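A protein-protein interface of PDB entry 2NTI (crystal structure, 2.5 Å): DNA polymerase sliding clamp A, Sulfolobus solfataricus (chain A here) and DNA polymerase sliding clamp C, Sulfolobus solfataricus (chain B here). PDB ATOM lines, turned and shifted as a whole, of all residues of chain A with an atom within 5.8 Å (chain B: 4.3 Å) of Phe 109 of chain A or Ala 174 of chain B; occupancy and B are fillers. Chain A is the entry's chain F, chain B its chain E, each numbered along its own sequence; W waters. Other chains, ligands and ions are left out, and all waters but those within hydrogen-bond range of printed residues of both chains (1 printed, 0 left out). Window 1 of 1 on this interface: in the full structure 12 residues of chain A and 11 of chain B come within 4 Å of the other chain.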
ATOM      1  N   TYR A  73      -0.885  22.256  13.861  1.00  0.00           N
ATOM      2  CA  TYR A  73      -0.123  22.460  12.639  1.00  0.00           C
ATOM      3  C   TYR A  73      -0.548  23.715  11.868  1.00  0.00           C
ATOM      4  O   TYR A  73       0.300  24.468  11.378  1.00  0.00           O
ATOM      5  CB  TYR A  73      -0.117  21.227  11.718  1.00  0.00           C
ATOM      6  CG  TYR A  73       0.988  21.381  10.701  1.00  0.00           C
ATOM      7  CD1 TYR A  73       2.318  21.093  11.048  1.00  0.00           C
ATOM      8  CD2 TYR A  73       0.735  21.909   9.426  1.00  0.00           C
ATOM      9  CE1 TYR A  73       3.369  21.288  10.143  1.00  0.00           C
ATOM     10  CE2 TYR A  73       1.780  22.108   8.512  1.00  0.00           C
ATOM     11  CZ  TYR A  73       3.098  21.791   8.878  1.00  0.00           C
ATOM     12  OH  TYR A  73       4.150  21.971   7.995  1.00  0.00           O
ATOM     13  N   ILE A  77       1.424  27.478  10.704  1.00  0.00           N
ATOM     14  CA  ILE A  77       1.361  28.131   9.407  1.00  0.00           C
ATOM     15  C   ILE A  77       0.883  29.577   9.538  1.00  0.00           C
ATOM     16  O   ILE A  77       1.465  30.473   8.945  1.00  0.00           O
ATOM     17  CB  ILE A  77       0.477  27.320   8.426  1.00  0.00           C
ATOM     18  CG1 ILE A  77       1.208  26.039   8.018  1.00  0.00           C
ATOM     19  CG2 ILE A  77       0.100  28.142   7.204  1.00  0.00           C
ATOM     20  CD1 ILE A  77       0.348  25.039   7.300  1.00  0.00           C
ATOM     21  N   VAL A  80       3.501  32.225  10.566  1.00  0.00           N
ATOM     22  CA  VAL A  80       4.549  32.667   9.642  1.00  0.00           C
ATOM     23  C   VAL A  80       4.209  34.043   9.054  1.00  0.00           C
ATOM     24  O   VAL A  80       5.045  34.660   8.393  1.00  0.00           O
ATOM     25  CB  VAL A  80       4.895  31.634   8.516  1.00  0.00           C
ATOM     26  CG1 VAL A  80       4.930  30.206   9.057  1.00  0.00           C
ATOM     27  CG2 VAL A  80       3.956  31.757   7.320  1.00  0.00           C
ATOM     28  N   VAL A  97      -4.517  20.402   0.123  1.00  0.00           N
ATOM     29  CA  VAL A  97      -4.881  21.803   0.293  1.00  0.00           C
ATOM     30  C   VAL A  97      -3.634  22.678   0.147  1.00  0.00           C
ATOM     31  O   VAL A  97      -2.572  22.345   0.680  1.00  0.00           O
ATOM     32  CB  VAL A  97      -5.607  22.033   1.637  1.00  0.00           C
ATOM     33  CG1 VAL A  97      -5.865  23.517   1.891  1.00  0.00           C
ATOM     34  CG2 VAL A  97      -6.916  21.265   1.657  1.00  0.00           C
ATOM     35  N   ILE A  98      -3.761  23.772  -0.607  1.00  0.00           N
ATOM     36  CA  ILE A  98      -2.661  24.713  -0.804  1.00  0.00           C
ATOM     37  C   ILE A  98      -2.904  25.973   0.006  1.00  0.00           C
ATOM     38  O   ILE A  98      -3.916  26.646  -0.180  1.00  0.00           O
ATOM     39  CB  ILE A  98      -2.479  25.112  -2.295  1.00  0.00           C
ATOM     40  CG1 ILE A  98      -2.244  23.883  -3.185  1.00  0.00           C
ATOM     41  CG2 ILE A  98      -1.335  26.118  -2.456  1.00  0.00           C
ATOM     42  CD1 ILE A  98      -0.834  23.234  -3.022  1.00  0.00           C
ATOM     43  N   ILE A  99      -1.972  26.283   0.907  1.00  0.00           N
ATOM     44  CA  ILE A  99      -2.008  27.538   1.650  1.00  0.00           C
ATOM     45  C   ILE A  99      -0.855  28.452   1.234  1.00  0.00           C
ATOM     46  O   ILE A  99       0.314  28.061   1.261  1.00  0.00           O
ATOM     47  CB  ILE A  99      -2.008  27.322   3.170  1.00  0.00           C
ATOM     48  CG1 ILE A  99      -3.255  26.535   3.587  1.00  0.00           C
ATOM     49  CG2 ILE A  99      -1.948  28.667   3.900  1.00  0.00           C
ATOM     50  CD1 ILE A  99      -3.128  25.802   4.905  1.00  0.00           C
ATOM     51  N   ASN A 100      -1.205  29.670   0.839  1.00  0.00           N
ATOM     52  CA  ASN A 100      -0.227  30.659   0.456  1.00  0.00           C
ATOM     53  C   ASN A 100      -0.274  31.842   1.388  1.00  0.00           C
ATOM     54  O   ASN A 100      -1.317  32.475   1.528  1.00  0.00           O
ATOM     55  CB  ASN A 100      -0.480  31.105  -0.979  1.00  0.00           C
ATOM     56  CG  ASN A 100       0.025  30.105  -1.989  1.00  0.00           C
ATOM     57  OD1 ASN A 100      -0.732  29.293  -2.505  1.00  0.00           O
ATOM     58  ND2 ASN A 100       1.318  30.142  -2.257  1.00  0.00           N
ATOM     59  N   ILE A 101       0.843  32.127   2.044  1.00  0.00           N
ATOM     60  CA  ILE A 101       0.955  33.338   2.844  1.00  0.00           C
ATOM     61  C   ILE A 101       1.645  34.392   1.998  1.00  0.00           C
ATOM     62  O   ILE A 101       2.832  34.275   1.667  1.00  0.00           O
ATOM     63  CB  ILE A 101       1.720  33.107   4.155  1.00  0.00           C
ATOM     64  CG1 ILE A 101       1.105  31.946   4.963  1.00  0.00           C
ATOM     65  CG2 ILE A 101       1.790  34.404   4.957  1.00  0.00           C
ATOM     66  CD1 ILE A 101      -0.320  32.178   5.452  1.00  0.00           C
ATOM     67  N   ARG A 107       4.989  32.431   0.911  1.00  0.00           N
ATOM     68  CA  ARG A 107       5.201  31.129   1.532  1.00  0.00           C
ATOM     69  C   ARG A 107       4.105  30.182   1.090  1.00  0.00           C
ATOM     70  O   ARG A 107       2.926  30.496   1.200  1.00  0.00           O
ATOM     71  CB  ARG A 107       5.249  31.247   3.053  1.00  0.00           C
ATOM     72  CG  ARG A 107       6.575  31.784   3.557  1.00  0.00           C
ATOM     73  CD  ARG A 107       6.635  33.289   3.444  1.00  0.00           C
ATOM     74  NE  ARG A 107       6.123  33.931   4.651  1.00  0.00           N
ATOM     75  CZ  ARG A 107       5.427  35.059   4.661  1.00  0.00           C
ATOM     76  NH1 ARG A 107       5.019  35.568   5.810  1.00  0.00           N
ATOM     77  NH2 ARG A 107       5.133  35.675   3.523  1.00  0.00           N
ATOM     78  N   GLU A 108       4.505  29.038   0.557  1.00  0.00           N
ATOM     79  CA  GLU A 108       3.546  28.066   0.088  1.00  0.00           C
ATOM     80  C   GLU A 108       3.568  26.823   0.957  1.00  0.00           C
ATOM     81  O   GLU A 108       4.621  26.240   1.208  1.00  0.00           O
ATOM     82  CB  GLU A 108       3.815  27.685  -1.371  1.00  0.00           C
ATOM     83  CG  GLU A 108       2.557  27.252  -2.113  1.00  0.00           C
ATOM     84  CD  GLU A 108       2.841  26.308  -3.265  1.00  0.00           C
ATOM     85  OE1 GLU A 108       2.947  25.081  -3.015  1.00  0.00           O
ATOM     86  OE2 GLU A 108       2.933  26.793  -4.418  1.00  0.00           O
ATOM     87  N   PHE A 109       2.392  26.411   1.402  1.00  0.00           N
ATOM     88  CA  PHE A 109       2.255  25.182   2.162  1.00  0.00           C
ATOM     89  C   PHE A 109       1.372  24.193   1.426  1.00  0.00           C
ATOM     90  O   PHE A 109       0.250  24.504   1.061  1.00  0.00           O
ATOM     91  CB  PHE A 109       1.702  25.484   3.553  1.00  0.00           C
ATOM     92  CG  PHE A 109       2.565  26.424   4.352  1.00  0.00           C
ATOM     93  CD1 PHE A 109       2.388  27.803   4.259  1.00  0.00           C
ATOM     94  CD2 PHE A 109       3.563  25.932   5.182  1.00  0.00           C
ATOM     95  CE1 PHE A 109       3.183  28.669   4.983  1.00  0.00           C
ATOM     96  CE2 PHE A 109       4.362  26.801   5.916  1.00  0.00           C
ATOM     97  CZ  PHE A 109       4.172  28.172   5.813  1.00  0.00           C
ATOM     98  N   ASN A 110       1.903  23.006   1.181  1.00  0.00           N
ATOM     99  CA  ASN A 110       1.109  21.926   0.623  1.00  0.00           C
ATOM    100  C   ASN A 110       0.710  20.977   1.750  1.00  0.00           C
ATOM    101  O   ASN A 110       1.536  20.264   2.293  1.00  0.00           O
ATOM    102  CB  ASN A 110       1.882  21.208  -0.484  1.00  0.00           C
ATOM    103  CG  ASN A 110       0.977  20.498  -1.464  1.00  0.00           C
ATOM    104  OD1 ASN A 110      -0.012  19.866  -1.072  1.00  0.00           O
ATOM    105  ND2 ASN A 110       1.318  20.594  -2.752  1.00  0.00           N
ATOM    106  N   VAL A 111      -0.565  21.009   2.110  1.00  0.00           N
ATOM    107  CA  VAL A 111      -1.093  20.226   3.233  1.00  0.00           C
ATOM    108  C   VAL A 111      -1.929  19.031   2.772  1.00  0.00           C
ATOM    109  O   VAL A 111      -2.815  19.170   1.922  1.00  0.00           O
ATOM    110  CB  VAL A 111      -1.992  21.088   4.167  1.00  0.00           C
ATOM    111  CG1 VAL A 111      -2.106  20.444   5.530  1.00  0.00           C
ATOM    112  CG2 VAL A 111      -1.437  22.493   4.316  1.00  0.00           C
ATOM    113  N   LEU B 147      10.709  29.278   8.518  1.00  0.00           N
ATOM    114  CA  LEU B 147      10.835  27.861   8.187  1.00  0.00           C
ATOM    115  C   LEU B 147      11.519  27.038   9.276  1.00  0.00           C
ATOM    116  O   LEU B 147      11.323  25.825   9.342  1.00  0.00           O
ATOM    117  CB  LEU B 147      11.585  27.678   6.860  1.00  0.00           C
ATOM    118  CG  LEU B 147      10.931  28.172   5.569  1.00  0.00           C
ATOM    119  CD1 LEU B 147      11.868  27.961   4.399  1.00  0.00           C
ATOM    120  CD2 LEU B 147       9.589  27.481   5.324  1.00  0.00           C
ATOM    121  N   LEU B 150       9.613  24.590  11.323  1.00  0.00           N
ATOM    122  CA  LEU B 150       8.829  23.623  10.569  1.00  0.00           C
ATOM    123  C   LEU B 150       9.536  22.307  10.274  1.00  0.00           C
ATOM    124  O   LEU B 150       8.931  21.410   9.698  1.00  0.00           O
ATOM    125  CB  LEU B 150       8.296  24.245   9.268  1.00  0.00           C
ATOM    126  CG  LEU B 150       7.630  25.630   9.343  1.00  0.00           C
ATOM    127  CD1 LEU B 150       7.200  26.073   7.973  1.00  0.00           C
ATOM    128  CD2 LEU B 150       6.442  25.674  10.288  1.00  0.00           C
ATOM    129  N   PHE B 165      13.609  27.256  -1.327  1.00  0.00           N
ATOM    130  CA  PHE B 165      13.752  26.723   0.025  1.00  0.00           C
ATOM    131  C   PHE B 165      12.555  25.833   0.344  1.00  0.00           C
ATOM    132  O   PHE B 165      11.407  26.240   0.160  1.00  0.00           O
ATOM    133  CB  PHE B 165      13.869  27.854   1.051  1.00  0.00           C
ATOM    134  CG  PHE B 165      15.149  28.630   0.955  1.00  0.00           C
ATOM    135  CD1 PHE B 165      15.300  29.830   1.643  1.00  0.00           C
ATOM    136  CD2 PHE B 165      16.211  28.175   0.172  1.00  0.00           C
ATOM    137  CE1 PHE B 165      16.497  30.558   1.564  1.00  0.00           C
ATOM    138  CE2 PHE B 165      17.399  28.905   0.082  1.00  0.00           C
ATOM    139  CZ  PHE B 165      17.540  30.098   0.780  1.00  0.00           C
ATOM    140  N   GLU B 166      12.837  24.617   0.803  1.00  0.00           N
ATOM    141  CA  GLU B 166      11.803  23.613   1.078  1.00  0.00           C
ATOM    142  C   GLU B 166      11.994  22.919   2.404  1.00  0.00           C
ATOM    143  O   GLU B 166      13.105  22.532   2.755  1.00  0.00           O
ATOM    144  CB  GLU B 166      11.801  22.541  -0.001  1.00  0.00           C
ATOM    145  CG  GLU B 166      10.725  22.682  -1.035  1.00  0.00           C
ATOM    146  CD  GLU B 166      10.907  21.714  -2.189  1.00  0.00           C
ATOM    147  OE1 GLU B 166      11.304  20.549  -1.948  1.00  0.00           O
ATOM    148  OE2 GLU B 166      10.657  22.118  -3.345  1.00  0.00           O
ATOM    149  N   VAL B 167      10.902  22.756   3.137  1.00  0.00           N
ATOM    150  CA  VAL B 167      10.899  21.881   4.305  1.00  0.00           C
ATOM    151  C   VAL B 167       9.805  20.851   4.123  1.00  0.00           C
ATOM    152  O   VAL B 167       8.625  21.200   4.037  1.00  0.00           O
ATOM    153  CB  VAL B 167      10.699  22.651   5.606  1.00  0.00           C
ATOM    154  CG1 VAL B 167      10.617  21.693   6.782  1.00  0.00           C
ATOM    155  CG2 VAL B 167      11.828  23.642   5.796  1.00  0.00           C
ATOM    156  N   THR B 173       4.257  20.389   3.421  1.00  0.00           N
ATOM    157  CA  THR B 173       5.506  20.723   2.776  1.00  0.00           C
ATOM    158  C   THR B 173       5.507  22.242   2.644  1.00  0.00           C
ATOM    159  O   THR B 173       4.524  22.830   2.204  1.00  0.00           O
ATOM    160  CB  THR B 173       5.634  19.958   1.410  1.00  0.00           C
ATOM    161  OG1 THR B 173       6.922  19.280   1.366  1.00  0.00           O
ATOM    162  CG2 THR B 173       5.520  20.877   0.210  1.00  0.00           C
ATOM    163  N   ALA B 174       6.582  22.881   3.081  1.00  0.00           N
ATOM    164  CA  ALA B 174       6.693  24.340   2.982  1.00  0.00           C
ATOM    165  C   ALA B 174       7.691  24.731   1.891  1.00  0.00           C
ATOM    166  O   ALA B 174       8.742  24.113   1.761  1.00  0.00           O
ATOM    167  CB  ALA B 174       7.095  24.937   4.316  1.00  0.00           C
ATOM    168  N   LYS B 175       7.359  25.748   1.108  1.00  0.00           N
ATOM    169  CA  LYS B 175       8.170  26.104  -0.044  1.00  0.00           C
ATOM    170  C   LYS B 175       8.199  27.607  -0.258  1.00  0.00           C
ATOM    171  O   LYS B 175       7.180  28.281  -0.095  1.00  0.00           O
ATOM    172  CB  LYS B 175       7.614  25.409  -1.281  1.00  0.00           C
ATOM    173  CG  LYS B 175       8.517  25.361  -2.501  1.00  0.00           C
ATOM    174  CD  LYS B 175       7.633  24.980  -3.688  1.00  0.00           C
ATOM    175  CE  LYS B 175       8.432  24.781  -4.958  1.00  0.00           C
ATOM    176  NZ  LYS B 175       7.545  25.172  -6.098  1.00  0.00           N
HETATM  177  O   HOH W   1       4.702  23.369  -0.845  1.00  0.00           O
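O of Glu 108 of chain A lies within hydrogen-bond range of N of Lys 175 of chain B.
The backbone carbonyl oxygen (O) of Thr 173 of chain B is in hydrogen-bond range of the backbone NH (N) of Asn 110 of chain A, at 2.8 Å.
N of Ala 174 of chain B sits at hydrogen-bond distance from O of Val 167 of chain B (2.8 Å).
The backbone carbonyl oxygen of Ile 99 of chain A is in hydrogen-bond range of the backbone NH of Phe 109 of chain A (2.7 Å).
The backbone carbonyl oxygen of Val 80 of chain A is in hydrogen-bond range of the guanidinium group of Arg 107 of chain A (2.7 Å).
The backbone NH (N) of Ile 101 of chain A is in hydrogen-bond range of the backbone carbonyl oxygen (O) of Arg 107 of chain A.
Among the printed residues, pairs that only touch across the chains: Phe 109 of chain A with Thr 173 of chain B, Glu 108 of chain A with Ala 174 of chain B, Glu 108 of chain A with Thr 173 of chain B, Phe 109 of chain A with Leu 150 of chain B, Phe 109 of chain A with Ala 174 of chain B and Arg 107 of chain A with Lys 175 of chain B.
Ala 174 of chain B touches just these residues of chain A: Glu 108 (3.3 Å) and Phe 109 (3.7 Å).
Printed residues of chain B within 4 Å of Glu 108 of chain A: Thr 173, Ala 174 and Lys 175.
Of the printed residues of chain B, Asn 110 of chain A touches Thr 173 (2.8 Å).
Asn 100 of chain A touches none of the printed residues of chain B.
Val 97 of chain A touches none of the printed residues of chain B.
The nearest residue of chain A that does not touch Ala 174 of chain B is Asn 110 of chain A (5.1 Å).
Of the 13 printed residues of chain A, 4 touch a printed residue of chain B.
Hydrophobic or aromatic side chains of chain A that line the printed part of chain B: Phe 109.
Of the 8 printed residues of chain B, 4 touch a printed residue of chain A.
Hydrophobic or aromatic side chains of chain B that line the printed part of chain A: Leu 150 and Ala 174.
Among the printed residues, no Asp or Glu carboxylate lies within 4 Å of a Lys or Arg side-chain nitrogen of the other chain.
Water W1 lies within hydrogen-bond range of the backbone carbonyl oxygen of Thr 173 of chain B (3.1 Å), the side-chain carboxylate of Glu 108 of chain A (3.3 Å) and the backbone NH of Asn 110 of chain A (3.5 Å).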
